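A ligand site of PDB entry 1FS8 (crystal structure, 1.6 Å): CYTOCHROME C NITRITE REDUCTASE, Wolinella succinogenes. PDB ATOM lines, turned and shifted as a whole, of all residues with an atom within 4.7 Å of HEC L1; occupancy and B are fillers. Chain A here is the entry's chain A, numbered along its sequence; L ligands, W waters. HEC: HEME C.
The backbone carbonyl oxygen of Ala 376 sits close to an oxygen (O2D) of HEC L1 (3.5 Å).
Residues that only touch HEC L1: Tyr 196, His 255, Pro 77, Asp 86, His 193, Asn 87, Cys 192, Tyr 74, Thr 90, Leu 104, His 378, Thr 93, Tyr 163, Phe 198, Val 216, Gln 191 and Ala 107.
Hydrophobic or aromatic side chains within 4 Å of HEC L1: Tyr 74, Pro 77, Leu 104, His 193, Tyr 196, Phe 198, Val 216, His 255 and His 378.
Of the 27 residues printed, 23 come within 4 Å of HEC L1.
The nearest printed residue that does not touch HEC L1 is Ala 76 (4.2 Å).
The side-chain sulfur (SG) of Cys 111 is in hydrogen-bond range of the side-chain hydroxyl (OH) of Tyr 163, at 3.3 Å.
ND2 of Asn 87 is in hydrogen-bond range of O of Cys 108 (3.2 Å).
A ring nitrogen (ND1) of His 255 is in hydrogen-bond range of the backbone carbonyl oxygen (O) of Val 194.
A ring nitrogen (ND1) of His 193 sits at hydrogen-bond distance from the side-chain carboxylate (OD2) of Asp 257 (2.6 Å).
The side-chain hydroxyl (OG1) of Thr 93 lies within hydrogen-bond range of the backbone carbonyl oxygen (O) of Asn 87 (3.1 Å).
OH of Tyr 74 lies within hydrogen-bond range of NE2 of His 378 (2.8 Å).
The backbone carbonyl oxygen of Gln 191 is in hydrogen-bond range of the side-chain hydroxyl of Tyr 163, at 2.6 Å.
O of Ala 107 lies within hydrogen-bond range of OG1 of Thr 110, 2.6 Å away.
SG of Cys 111 is bonded to CAC of HEC L1 (1.8 Å).
SG of Cys 108 is covalently linked to CAB of HEC L1, 1.9 Å away.
The side-chain amino group of Lys 112 is bound to an iron atom (FE) of HEC L1, 2.1 Å away.
The guanidinium group (NH1) of Arg 92 lies within salt-bridge range of an oxygen (O2A) of HEC L1.
An oxygen (O1A) of HEC L1 is in hydrogen-bond range of the backbone NH (N) of Asn 75 (3.1 Å).
An oxygen (O2D) of HEC L2 lies close to the side-chain carboxylate of Asp 86.
An iron atom (FE) of HEC L2 is bound by a ring nitrogen (NE2) of His 193.
CAC of HEC L2 is covalently linked to SG of Cys 192, at 1.8 Å.
Water W8 lies within hydrogen-bond range of an oxygen (O2D) of HEC L1 (2.6 Å), the backbone carbonyl oxygen (O) of Ala 376 (2.7 Å) and the side-chain hydroxyl (OH) of Tyr 74 (2.7 Å).
Water W7 bridges an oxygen (O1A) of HEC L1 and the side-chain amide nitrogen (ND2) of Asn 75.
Water W4 lies within hydrogen-bond range of OG1 of Thr 90, O1A of HEC L1, NH1 of Arg 92 and ND2 of Asn 75.
Water W3 lies within hydrogen-bond range of the backbone carbonyl oxygen (O) of Asn 75 (2.8 Å), an oxygen (O1D) of HEC L1 (2.8 Å), a ring nitrogen (NE2) of His 378 (3.1 Å) and the side-chain hydroxyl (OH) of Tyr 74 (3.2 Å).
Water W9 lies within hydrogen-bond range of N of His 378 (2.8 Å), O2D of HEC L1 (2.8 Å) and OD1 of Asp 257 (2.9 Å).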
ATOM      1  N   TYR A  74      31.737   5.614  16.976  1.00  0.00           N
ATOM      2  CA  TYR A  74      30.883   5.740  18.158  1.00  0.00           C
ATOM      3  C   TYR A  74      31.236   4.628  19.126  1.00  0.00           C
ATOM      4  O   TYR A  74      30.982   3.458  18.851  1.00  0.00           O
ATOM      5  CB  TYR A  74      29.404   5.636  17.804  1.00  0.00           C
ATOM      6  CG  TYR A  74      28.501   5.650  19.027  1.00  0.00           C
ATOM      7  CD1 TYR A  74      28.540   6.710  19.938  1.00  0.00           C
ATOM      8  CD2 TYR A  74      27.636   4.589  19.300  1.00  0.00           C
ATOM      9  CE1 TYR A  74      27.733   6.719  21.076  1.00  0.00           C
ATOM     10  CE2 TYR A  74      26.827   4.583  20.430  1.00  0.00           C
ATOM     11  CZ  TYR A  74      26.889   5.655  21.314  1.00  0.00           C
ATOM     12  OH  TYR A  74      26.103   5.642  22.449  1.00  0.00           O
ATOM     13  N   ASN A  75      31.806   5.005  20.261  1.00  0.00           N
ATOM     14  CA  ASN A  75      32.201   4.040  21.280  1.00  0.00           C
ATOM     15  C   ASN A  75      31.458   4.281  22.582  1.00  0.00           C
ATOM     16  O   ASN A  75      30.911   5.372  22.794  1.00  0.00           O
ATOM     17  CB  ASN A  75      33.708   4.143  21.534  1.00  0.00           C
ATOM     18  CG  ASN A  75      34.512   4.153  20.261  1.00  0.00           C
ATOM     19  OD1 ASN A  75      34.319   3.301  19.391  1.00  0.00           O
ATOM     20  ND2 ASN A  75      35.423   5.112  20.128  1.00  0.00           N
ATOM     21  N   ALA A  76      31.444   3.280  23.442  1.00  0.00           N
ATOM     22  CA  ALA A  76      30.784   3.379  24.735  1.00  0.00           C
ATOM     23  C   ALA A  76      31.618   4.319  25.601  1.00  0.00           C
ATOM     24  O   ALA A  76      32.798   4.553  25.325  1.00  0.00           O
ATOM     25  CB  ALA A  76      30.695   2.016  25.383  1.00  0.00           C
ATOM     26  N   PRO A  77      31.024   4.869  26.659  1.00  0.00           N
ATOM     27  CA  PRO A  77      31.741   5.775  27.555  1.00  0.00           C
ATOM     28  C   PRO A  77      32.788   5.039  28.371  1.00  0.00           C
ATOM     29  O   PRO A  77      32.606   3.871  28.708  1.00  0.00           O
ATOM     30  CB  PRO A  77      30.649   6.312  28.474  1.00  0.00           C
ATOM     31  CG  PRO A  77      29.376   6.033  27.745  1.00  0.00           C
ATOM     32  CD  PRO A  77      29.625   4.723  27.083  1.00  0.00           C
ATOM     33  N   ASP A  86      39.494  11.404  23.960  1.00  0.00           N
ATOM     34  CA  ASP A  86      38.551  10.692  23.113  1.00  0.00           C
ATOM     35  C   ASP A  86      37.844  11.663  22.188  1.00  0.00           C
ATOM     36  O   ASP A  86      37.501  11.337  21.057  1.00  0.00           O
ATOM     37  CB  ASP A  86      37.548   9.913  23.955  1.00  0.00           C
ATOM     38  CG  ASP A  86      38.153   8.678  24.584  1.00  0.00           C
ATOM     39  OD1 ASP A  86      39.224   8.250  24.094  1.00  0.00           O
ATOM     40  OD2 ASP A  86      37.581   8.129  25.543  1.00  0.00           O
ATOM     41  N   ASN A  87      37.637  12.883  22.692  1.00  0.00           N
ATOM     42  CA  ASN A  87      37.010  13.936  21.917  1.00  0.00           C
ATOM     43  C   ASN A  87      37.932  14.243  20.728  1.00  0.00           C
ATOM     44  O   ASN A  87      37.483  14.485  19.611  1.00  0.00           O
ATOM     45  CB  ASN A  87      36.853  15.172  22.820  1.00  0.00           C
ATOM     46  CG  ASN A  87      36.125  16.309  22.135  1.00  0.00           C
ATOM     47  OD1 ASN A  87      36.636  17.419  22.055  1.00  0.00           O
ATOM     48  ND2 ASN A  87      34.900  16.050  21.672  1.00  0.00           N
ATOM     49  N   THR A  90      38.110  10.638  18.348  1.00  0.00           N
ATOM     50  CA  THR A  90      36.969  10.199  17.569  1.00  0.00           C
ATOM     51  C   THR A  90      37.000  10.704  16.133  1.00  0.00           C
ATOM     52  O   THR A  90      37.325  11.870  15.877  1.00  0.00           O
ATOM     53  CB  THR A  90      35.635  10.629  18.203  1.00  0.00           C
ATOM     54  OG1 THR A  90      34.565  10.139  17.391  1.00  0.00           O
ATOM     55  CG2 THR A  90      35.543  12.138  18.288  1.00  0.00           C
ATOM     56  N   ARG A  92      34.660  11.474  14.517  1.00  0.00           N
ATOM     57  CA  ARG A  92      33.634  12.493  14.365  1.00  0.00           C
ATOM     58  C   ARG A  92      34.199  13.908  14.280  1.00  0.00           C
ATOM     59  O   ARG A  92      33.651  14.747  13.575  1.00  0.00           O
ATOM     60  CB  ARG A  92      32.608  12.402  15.501  1.00  0.00           C
ATOM     61  CG  ARG A  92      31.954  11.024  15.604  1.00  0.00           C
ATOM     62  CD  ARG A  92      30.559  11.090  16.217  1.00  0.00           C
ATOM     63  NE  ARG A  92      30.525  11.574  17.591  1.00  0.00           N
ATOM     64  CZ  ARG A  92      30.812  10.832  18.660  1.00  0.00           C
ATOM     65  NH1 ARG A  92      31.164   9.568  18.527  1.00  0.00           N
ATOM     66  NH2 ARG A  92      30.705  11.353  19.873  1.00  0.00           N
ATOM     67  N   THR A  93      35.306  14.185  14.987  1.00  0.00           N
ATOM     68  CA  THR A  93      35.883  15.523  14.925  1.00  0.00           C
ATOM     69  C   THR A  93      36.799  15.715  13.716  1.00  0.00           C
ATOM     70  O   THR A  93      37.349  16.786  13.495  1.00  0.00           O
ATOM     71  CB  THR A  93      36.664  15.870  16.219  1.00  0.00           C
ATOM     72  OG1 THR A  93      37.532  14.779  16.569  1.00  0.00           O
ATOM     73  CG2 THR A  93      35.682  16.127  17.370  1.00  0.00           C
ATOM     74  N   LEU A 104      33.402  19.756  12.868  1.00  0.00           N
ATOM     75  CA  LEU A 104      32.603  20.177  14.015  1.00  0.00           C
ATOM     76  C   LEU A 104      32.925  21.523  14.663  1.00  0.00           C
ATOM     77  O   LEU A 104      34.030  22.043  14.517  1.00  0.00           O
ATOM     78  CB  LEU A 104      32.648  19.049  15.067  1.00  0.00           C
ATOM     79  CG  LEU A 104      32.176  17.700  14.497  1.00  0.00           C
ATOM     80  CD1 LEU A 104      32.207  16.638  15.578  1.00  0.00           C
ATOM     81  CD2 LEU A 104      30.767  17.837  13.934  1.00  0.00           C
ATOM     82  N   ALA A 107      31.568  23.969  20.242  1.00  0.00           N
ATOM     83  CA  ALA A 107      30.702  23.403  21.282  1.00  0.00           C
ATOM     84  C   ALA A 107      31.064  21.972  21.664  1.00  0.00           C
ATOM     85  O   ALA A 107      30.693  21.503  22.734  1.00  0.00           O
ATOM     86  CB  ALA A 107      29.242  23.471  20.850  1.00  0.00           C
ATOM     87  N   CYS A 108      31.787  21.281  20.792  1.00  0.00           N
ATOM     88  CA  CYS A 108      32.175  19.901  21.092  1.00  0.00           C
ATOM     89  C   CYS A 108      33.145  19.750  22.254  1.00  0.00           C
ATOM     90  O   CYS A 108      33.361  18.638  22.739  1.00  0.00           O
ATOM     91  CB  CYS A 108      32.719  19.208  19.830  1.00  0.00           C
ATOM     92  SG  CYS A 108      31.406  18.747  18.660  1.00  0.00           S
ATOM     93  N   THR A 110      32.785  21.590  25.128  1.00  0.00           N
ATOM     94  CA  THR A 110      31.949  21.919  26.280  1.00  0.00           C
ATOM     95  C   THR A 110      31.876  20.978  27.470  1.00  0.00           C
ATOM     96  O   THR A 110      32.035  21.403  28.617  1.00  0.00           O
ATOM     97  CB  THR A 110      30.515  22.240  25.823  1.00  0.00           C
ATOM     98  OG1 THR A 110      30.575  23.153  24.731  1.00  0.00           O
ATOM     99  CG2 THR A 110      29.717  22.873  26.964  1.00  0.00           C
ATOM    100  N   CYS A 111      31.632  19.703  27.211  1.00  0.00           N
ATOM    101  CA  CYS A 111      31.501  18.748  28.313  1.00  0.00           C
ATOM    102  C   CYS A 111      32.685  17.804  28.422  1.00  0.00           C
ATOM    103  O   CYS A 111      32.535  16.657  28.832  1.00  0.00           O
ATOM    104  CB  CYS A 111      30.213  17.949  28.131  1.00  0.00           C
ATOM    105  SG  CYS A 111      28.754  18.976  27.833  1.00  0.00           S
ATOM    106  N   LYS A 112      33.869  18.303  28.084  1.00  0.00           N
ATOM    107  CA  LYS A 112      35.061  17.475  28.132  1.00  0.00           C
ATOM    108  C   LYS A 112      36.201  18.078  28.930  1.00  0.00           C
ATOM    109  O   LYS A 112      37.191  17.400  29.189  1.00  0.00           O
ATOM    110  CB  LYS A 112      35.573  17.224  26.710  1.00  0.00           C
ATOM    111  CG  LYS A 112      34.545  16.673  25.738  1.00  0.00           C
ATOM    112  CD  LYS A 112      34.249  15.219  26.040  1.00  0.00           C
ATOM    113  CE  LYS A 112      33.290  14.629  25.023  1.00  0.00           C
ATOM    114  NZ  LYS A 112      31.924  15.230  25.085  1.00  0.00           N
ATOM    115  N   TYR A 163      23.625  26.872  30.158  1.00  0.00           N
ATOM    116  CA  TYR A 163      22.525  26.188  29.501  1.00  0.00           C
ATOM    117  C   TYR A 163      21.766  25.215  30.402  1.00  0.00           C
ATOM    118  O   TYR A 163      20.609  24.892  30.133  1.00  0.00           O
ATOM    119  CB  TYR A 163      23.007  25.465  28.225  1.00  0.00           C
ATOM    120  CG  TYR A 163      24.081  24.415  28.430  1.00  0.00           C
ATOM    121  CD1 TYR A 163      23.780  23.189  29.036  1.00  0.00           C
ATOM    122  CD2 TYR A 163      25.394  24.655  28.040  1.00  0.00           C
ATOM    123  CE1 TYR A 163      24.759  22.230  29.236  1.00  0.00           C
ATOM    124  CE2 TYR A 163      26.385  23.695  28.227  1.00  0.00           C
ATOM    125  CZ  TYR A 163      26.061  22.489  28.827  1.00  0.00           C
ATOM    126  OH  TYR A 163      27.040  21.544  29.026  1.00  0.00           O
ATOM    127  N   GLN A 191      25.320  18.680  33.964  1.00  0.00           N
ATOM    128  CA  GLN A 191      25.918  19.722  33.147  1.00  0.00           C
ATOM    129  C   GLN A 191      26.310  19.102  31.823  1.00  0.00           C
ATOM    130  O   GLN A 191      26.329  19.770  30.789  1.00  0.00           O
ATOM    131  CB  GLN A 191      27.201  20.264  33.782  1.00  0.00           C
ATOM    132  CG  GLN A 191      27.072  20.942  35.111  1.00  0.00           C
ATOM    133  CD  GLN A 191      28.422  21.431  35.600  1.00  0.00           C
ATOM    134  OE1 GLN A 191      28.914  22.456  35.139  1.00  0.00           O
ATOM    135  NE2 GLN A 191      29.038  20.671  36.500  1.00  0.00           N
ATOM    136  N   CYS A 192      26.638  17.816  31.862  1.00  0.00           N
ATOM    137  CA  CYS A 192      27.092  17.093  30.685  1.00  0.00           C
ATOM    138  C   CYS A 192      26.272  15.869  30.291  1.00  0.00           C
ATOM    139  O   CYS A 192      26.098  15.604  29.105  1.00  0.00           O
ATOM    140  CB  CYS A 192      28.528  16.633  30.884  1.00  0.00           C
ATOM    141  SG  CYS A 192      29.635  17.941  31.442  1.00  0.00           S
ATOM    142  N   HIS A 193      25.799  15.132  31.282  1.00  0.00           N
ATOM    143  CA  HIS A 193      25.042  13.905  31.037  1.00  0.00           C
ATOM    144  C   HIS A 193      23.571  14.152  30.728  1.00  0.00           C
ATOM    145  O   HIS A 193      22.674  13.652  31.421  1.00  0.00           O
ATOM    146  CB  HIS A 193      25.204  12.965  32.233  1.00  0.00           C
ATOM    147  CG  HIS A 193      26.547  12.310  32.294  1.00  0.00           C
ATOM    148  ND1 HIS A 193      26.864  11.136  31.637  1.00  0.00           N
ATOM    149  CD2 HIS A 193      27.697  12.700  32.899  1.00  0.00           C
ATOM    150  CE1 HIS A 193      28.154  10.867  31.856  1.00  0.00           C
ATOM    151  NE2 HIS A 193      28.710  11.791  32.624  1.00  0.00           N
ATOM    152  N   VAL A 194      23.337  14.916  29.665  1.00  0.00           N
ATOM    153  CA  VAL A 194      21.988  15.246  29.228  1.00  0.00           C
ATOM    154  C   VAL A 194      21.934  15.304  27.702  1.00  0.00           C
ATOM    155  O   VAL A 194      22.978  15.352  27.039  1.00  0.00           O
ATOM    156  CB  VAL A 194      21.551  16.631  29.764  1.00  0.00           C
ATOM    157  CG1 VAL A 194      21.325  16.571  31.275  1.00  0.00           C
ATOM    158  CG2 VAL A 194      22.617  17.674  29.424  1.00  0.00           C
ATOM    159  N   TYR A 196      21.058  17.174  24.163  1.00  0.00           N
ATOM    160  CA  TYR A 196      21.146  18.560  23.720  1.00  0.00           C
ATOM    161  C   TYR A 196      21.114  18.639  22.196  1.00  0.00           C
ATOM    162  O   TYR A 196      21.105  17.631  21.501  1.00  0.00           O
ATOM    163  CB  TYR A 196      22.469  19.168  24.185  1.00  0.00           C
ATOM    164  CG  TYR A 196      23.639  18.585  23.416  1.00  0.00           C
ATOM    165  CD1 TYR A 196      24.189  17.343  23.750  1.00  0.00           C
ATOM    166  CD2 TYR A 196      24.126  19.219  22.275  1.00  0.00           C
ATOM    167  CE1 TYR A 196      25.180  16.744  22.962  1.00  0.00           C
ATOM    168  CE2 TYR A 196      25.108  18.627  21.479  1.00  0.00           C
ATOM    169  CZ  TYR A 196      25.633  17.400  21.827  1.00  0.00           C
ATOM    170  OH  TYR A 196      26.582  16.820  21.017  1.00  0.00           O
ATOM    171  N   PHE A 198      22.366  21.805  18.985  1.00  0.00           N
ATOM    172  CA  PHE A 198      23.048  23.075  18.760  1.00  0.00           C
ATOM    173  C   PHE A 198      22.077  24.053  18.134  1.00  0.00           C
ATOM    174  O   PHE A 198      21.489  23.768  17.099  1.00  0.00           O
ATOM    175  CB  PHE A 198      24.235  22.913  17.821  1.00  0.00           C
ATOM    176  CG  PHE A 198      25.347  22.057  18.364  1.00  0.00           C
ATOM    177  CD1 PHE A 198      25.715  22.122  19.704  1.00  0.00           C
ATOM    178  CD2 PHE A 198      26.046  21.198  17.521  1.00  0.00           C
ATOM    179  CE1 PHE A 198      26.765  21.355  20.193  1.00  0.00           C
ATOM    180  CE2 PHE A 198      27.100  20.422  17.999  1.00  0.00           C
ATOM    181  CZ  PHE A 198      27.461  20.494  19.340  1.00  0.00           C
ATOM    182  N   VAL A 216      24.945  25.164  22.750  1.00  0.00           N
ATOM    183  CA  VAL A 216      24.401  23.952  23.371  1.00  0.00           C
ATOM    184  C   VAL A 216      23.080  24.340  24.005  1.00  0.00           C
ATOM    185  O   VAL A 216      23.005  25.278  24.808  1.00  0.00           O
ATOM    186  CB  VAL A 216      25.354  23.405  24.454  1.00  0.00           C
ATOM    187  CG1 VAL A 216      24.685  22.275  25.222  1.00  0.00           C
ATOM    188  CG2 VAL A 216      26.634  22.910  23.807  1.00  0.00           C
ATOM    189  N   HIS A 255      23.257  10.795  25.015  1.00  0.00           N
ATOM    190  CA  HIS A 255      23.323  10.539  26.451  1.00  0.00           C
ATOM    191  C   HIS A 255      22.357  11.315  27.333  1.00  0.00           C
ATOM    192  O   HIS A 255      22.763  12.209  28.087  1.00  0.00           O
ATOM    193  CB  HIS A 255      24.765  10.814  26.913  1.00  0.00           C
ATOM    194  CG  HIS A 255      25.367  12.026  26.289  1.00  0.00           C
ATOM    195  ND1 HIS A 255      24.916  13.298  26.558  1.00  0.00           N
ATOM    196  CD2 HIS A 255      26.343  12.161  25.368  1.00  0.00           C
ATOM    197  CE1 HIS A 255      25.579  14.168  25.811  1.00  0.00           C
ATOM    198  NE2 HIS A 255      26.451  13.502  25.077  1.00  0.00           N
ATOM    199  N   ASP A 257      21.239  10.864  30.042  1.00  0.00           N
ATOM    200  CA  ASP A 257      21.360  10.156  31.302  1.00  0.00           C
ATOM    201  C   ASP A 257      20.507  10.710  32.431  1.00  0.00           C
ATOM    202  O   ASP A 257      19.779   9.960  33.082  1.00  0.00           O
ATOM    203  CB  ASP A 257      22.824  10.132  31.751  1.00  0.00           C
ATOM    204  CG  ASP A 257      23.757   9.666  30.648  1.00  0.00           C
ATOM    205  OD1 ASP A 257      23.532   8.567  30.093  1.00  0.00           O
ATOM    206  OD2 ASP A 257      24.717  10.406  30.335  1.00  0.00           O
ATOM    207  N   ALA A 376      20.821   5.704  24.014  1.00  0.00           N
ATOM    208  CA  ALA A 376      21.927   6.656  24.063  1.00  0.00           C
ATOM    209  C   ALA A 376      22.507   6.847  25.467  1.00  0.00           C
ATOM    210  O   ALA A 376      23.671   7.210  25.607  1.00  0.00           O
ATOM    211  CB  ALA A 376      21.486   8.001  23.479  1.00  0.00           C
ATOM    212  N   HIS A 378      23.839   5.049  28.315  1.00  0.00           N
ATOM    213  CA  HIS A 378      24.322   3.696  28.590  1.00  0.00           C
ATOM    214  C   HIS A 378      23.957   3.054  29.909  1.00  0.00           C
ATOM    215  O   HIS A 378      24.089   1.840  30.071  1.00  0.00           O
ATOM    216  CB  HIS A 378      25.834   3.666  28.378  1.00  0.00           C
ATOM    217  CG  HIS A 378      26.230   3.726  26.941  1.00  0.00           C
ATOM    218  ND1 HIS A 378      26.326   2.597  26.147  1.00  0.00           N
ATOM    219  CD2 HIS A 378      26.463   4.779  26.117  1.00  0.00           C
ATOM    220  CE1 HIS A 378      26.615   2.955  24.919  1.00  0.00           C
ATOM    221  NE2 HIS A 378      26.708   4.271  24.871  1.00  0.00           N
HETATM  222 FE   HEC L   1      30.418  14.244  24.021  1.00  0.00          FE
HETATM  223  CHA HEC L   1      31.003  11.142  25.279  1.00  0.00           C
HETATM  224  CHB HEC L   1      32.484  13.609  21.416  1.00  0.00           C
HETATM  225  CHC HEC L   1      29.401  17.130  22.542  1.00  0.00           C
HETATM  226  CHD HEC L   1      28.691  15.052  26.822  1.00  0.00           C
HETATM  227  NA  HEC L   1      31.568  12.722  23.492  1.00  0.00           N
HETATM  228  C1A HEC L   1      31.714  11.515  24.145  1.00  0.00           C
HETATM  229  C2A HEC L   1      32.711  10.678  23.487  1.00  0.00           C
HETATM  230  C3A HEC L   1      33.124  11.373  22.400  1.00  0.00           C
HETATM  231  C4A HEC L   1      32.398  12.631  22.395  1.00  0.00           C
HETATM  232  CMA HEC L   1      34.147  10.926  21.367  1.00  0.00           C
HETATM  233  CAA HEC L   1      33.117   9.266  23.929  1.00  0.00           C
HETATM  234  CBA HEC L   1      32.100   8.232  23.433  1.00  0.00           C
HETATM  235  CGA HEC L   1      31.998   8.213  21.923  1.00  0.00           C
HETATM  236  O1A HEC L   1      32.936   7.708  21.275  1.00  0.00           O
HETATM  237  O2A HEC L   1      30.984   8.700  21.385  1.00  0.00           O
HETATM  238  NB  HEC L   1      30.865  15.187  22.351  1.00  0.00           N
HETATM  239  C1B HEC L   1      31.754  14.772  21.368  1.00  0.00           C
HETATM  240  C2B HEC L   1      31.683  15.637  20.218  1.00  0.00           C
HETATM  241  C3B HEC L   1      30.768  16.602  20.476  1.00  0.00           C
HETATM  242  C4B HEC L   1      30.283  16.330  21.826  1.00  0.00           C
HETATM  243  CMB HEC L   1      32.495  15.475  18.925  1.00  0.00           C
HETATM  244  CAB HEC L   1      30.299  17.575  19.576  1.00  0.00           C
HETATM  245  CBB HEC L   1      29.318  17.209  18.610  1.00  0.00           C
HETATM  246  NC  HEC L   1      29.274  15.754  24.571  1.00  0.00           N
HETATM  247  C1C HEC L   1      28.954  16.875  23.831  1.00  0.00           C
HETATM  248  C2C HEC L   1      28.220  17.832  24.645  1.00  0.00           C
HETATM  249  C3C HEC L   1      28.047  17.291  25.880  1.00  0.00           C
HETATM  250  C4C HEC L   1      28.673  15.976  25.799  1.00  0.00           C
HETATM  251  CMC HEC L   1      27.766  19.219  24.154  1.00  0.00           C
HETATM  252  CAC HEC L   1      27.513  17.912  27.032  1.00  0.00           C
HETATM  253  CBC HEC L   1      26.252  18.566  27.044  1.00  0.00           C
HETATM  254  ND  HEC L   1      29.922  13.285  25.663  1.00  0.00           N
HETATM  255  C1D HEC L   1      29.202  13.779  26.744  1.00  0.00           C
HETATM  256  C2D HEC L   1      28.946  12.750  27.716  1.00  0.00           C
HETATM  257  C3D HEC L   1      29.497  11.624  27.217  1.00  0.00           C
HETATM  258  C4D HEC L   1      30.148  11.969  25.986  1.00  0.00           C
HETATM  259  CMD HEC L   1      28.210  12.895  29.054  1.00  0.00           C
HETATM  260  CAD HEC L   1      29.540  10.290  27.965  1.00  0.00           C
HETATM  261  CBD HEC L   1      28.299   9.397  27.955  1.00  0.00           C
HETATM  262  CGD HEC L   1      28.021   8.792  26.592  1.00  0.00           C
HETATM  263  O1D HEC L   1      28.938   8.790  25.737  1.00  0.00           O
HETATM  264  O2D HEC L   1      26.899   8.297  26.390  1.00  0.00           O
HETATM  265 FE   HEC L   2      30.599  11.690  33.339  1.00  0.00          FE
HETATM  266  CHA HEC L   2      31.796   9.213  31.303  1.00  0.00           C
HETATM  267  CHB HEC L   2      29.136   9.423  35.297  1.00  0.00           C
HETATM  268  CHC HEC L   2      29.880  14.148  35.582  1.00  0.00           C
HETATM  269  CHD HEC L   2      31.413  14.012  31.026  1.00  0.00           C
HETATM  270  NA  HEC L   2      30.526   9.731  33.317  1.00  0.00           N
HETATM  271  C1A HEC L   2      31.174   8.835  32.478  1.00  0.00           C
HETATM  272  C2A HEC L   2      30.968   7.476  32.907  1.00  0.00           C
HETATM  273  C3A HEC L   2      30.144   7.532  34.004  1.00  0.00           C
HETATM  274  C4A HEC L   2      29.865   8.936  34.223  1.00  0.00           C
HETATM  275  CMA HEC L   2      29.703   6.367  34.875  1.00  0.00           C
HETATM  276  CAA HEC L   2      31.595   6.235  32.274  1.00  0.00           C
HETATM  277  CBA HEC L   2      32.555   5.596  33.269  1.00  0.00           C
HETATM  278  CGA HEC L   2      33.244   4.374  32.713  1.00  0.00           C
HETATM  279  O1A HEC L   2      32.730   3.804  31.733  1.00  0.00           O
HETATM  280  O2A HEC L   2      34.283   3.980  33.259  1.00  0.00           O
HETATM  281  NB  HEC L   2      29.705  11.786  35.089  1.00  0.00           N
HETATM  282  C1B HEC L   2      29.091  10.739  35.745  1.00  0.00           C
HETATM  283  C2B HEC L   2      28.519  11.168  36.992  1.00  0.00           C
HETATM  284  C3B HEC L   2      28.781  12.506  37.139  1.00  0.00           C
HETATM  285  C4B HEC L   2      29.524  12.867  35.927  1.00  0.00           C
HETATM  286  CMB HEC L   2      27.774  10.252  37.979  1.00  0.00           C
HETATM  287  CAB HEC L   2      28.464  13.349  38.213  1.00  0.00           C
HETATM  288  CBB HEC L   2      28.945  13.150  39.525  1.00  0.00           C
HETATM  289  NC  HEC L   2      30.671  13.652  33.320  1.00  0.00           N
HETATM  290  C1C HEC L   2      30.387  14.521  34.352  1.00  0.00           C
HETATM  291  C2C HEC L   2      30.580  15.890  33.957  1.00  0.00           C
HETATM  292  C3C HEC L   2      30.958  15.896  32.662  1.00  0.00           C
HETATM  293  C4C HEC L   2      31.021  14.491  32.267  1.00  0.00           C
HETATM  294  CMC HEC L   2      30.392  17.105  34.880  1.00  0.00           C
HETATM  295  CAC HEC L   2      31.170  17.036  31.867  1.00  0.00           C
HETATM  296  CBC HEC L   2      32.124  18.032  32.226  1.00  0.00           C
HETATM  297  ND  HEC L   2      31.362  11.631  31.524  1.00  0.00           N
HETATM  298  C1D HEC L   2      31.598  12.690  30.679  1.00  0.00           C
HETATM  299  C2D HEC L   2      32.257  12.256  29.463  1.00  0.00           C
HETATM  300  C3D HEC L   2      32.408  10.917  29.558  1.00  0.00           C
HETATM  301  C4D HEC L   2      31.828  10.510  30.818  1.00  0.00           C
HETATM  302  CMD HEC L   2      32.638  13.120  28.257  1.00  0.00           C
HETATM  303  CAD HEC L   2      33.043  10.046  28.473  1.00  0.00           C
HETATM  304  CBD HEC L   2      34.501   9.757  28.789  1.00  0.00           C
HETATM  305  CGD HEC L   2      35.183   8.991  27.685  1.00  0.00           C
HETATM  306  O1D HEC L   2      34.561   8.068  27.128  1.00  0.00           O
HETATM  307  O2D HEC L   2      36.349   9.314  27.374  1.00  0.00           O
HETATM  308  O   HOH W   1      28.905  10.017  22.943  1.00  0.00           O
HETATM  309  O   HOH W   2      31.559  18.199  24.796  1.00  0.00           O
HETATM  310  O   HOH W   3      28.732   6.482  24.155  1.00  0.00           O
HETATM  311  O   HOH W   4      33.877   7.842  18.693  1.00  0.00           O
HETATM  312  O   HOH W   5      35.038  11.638  25.605  1.00  0.00           O
HETATM  313  O   HOH W   6      29.343  13.904  18.212  1.00  0.00           O
HETATM  314  O   HOH W   7      35.481   7.247  22.170  1.00  0.00           O
HETATM  315  O   HOH W   8      25.771   7.731  24.072  1.00  0.00           O
HETATM  316  O   HOH W   9      25.593   7.216  28.645  1.00  0.00           O
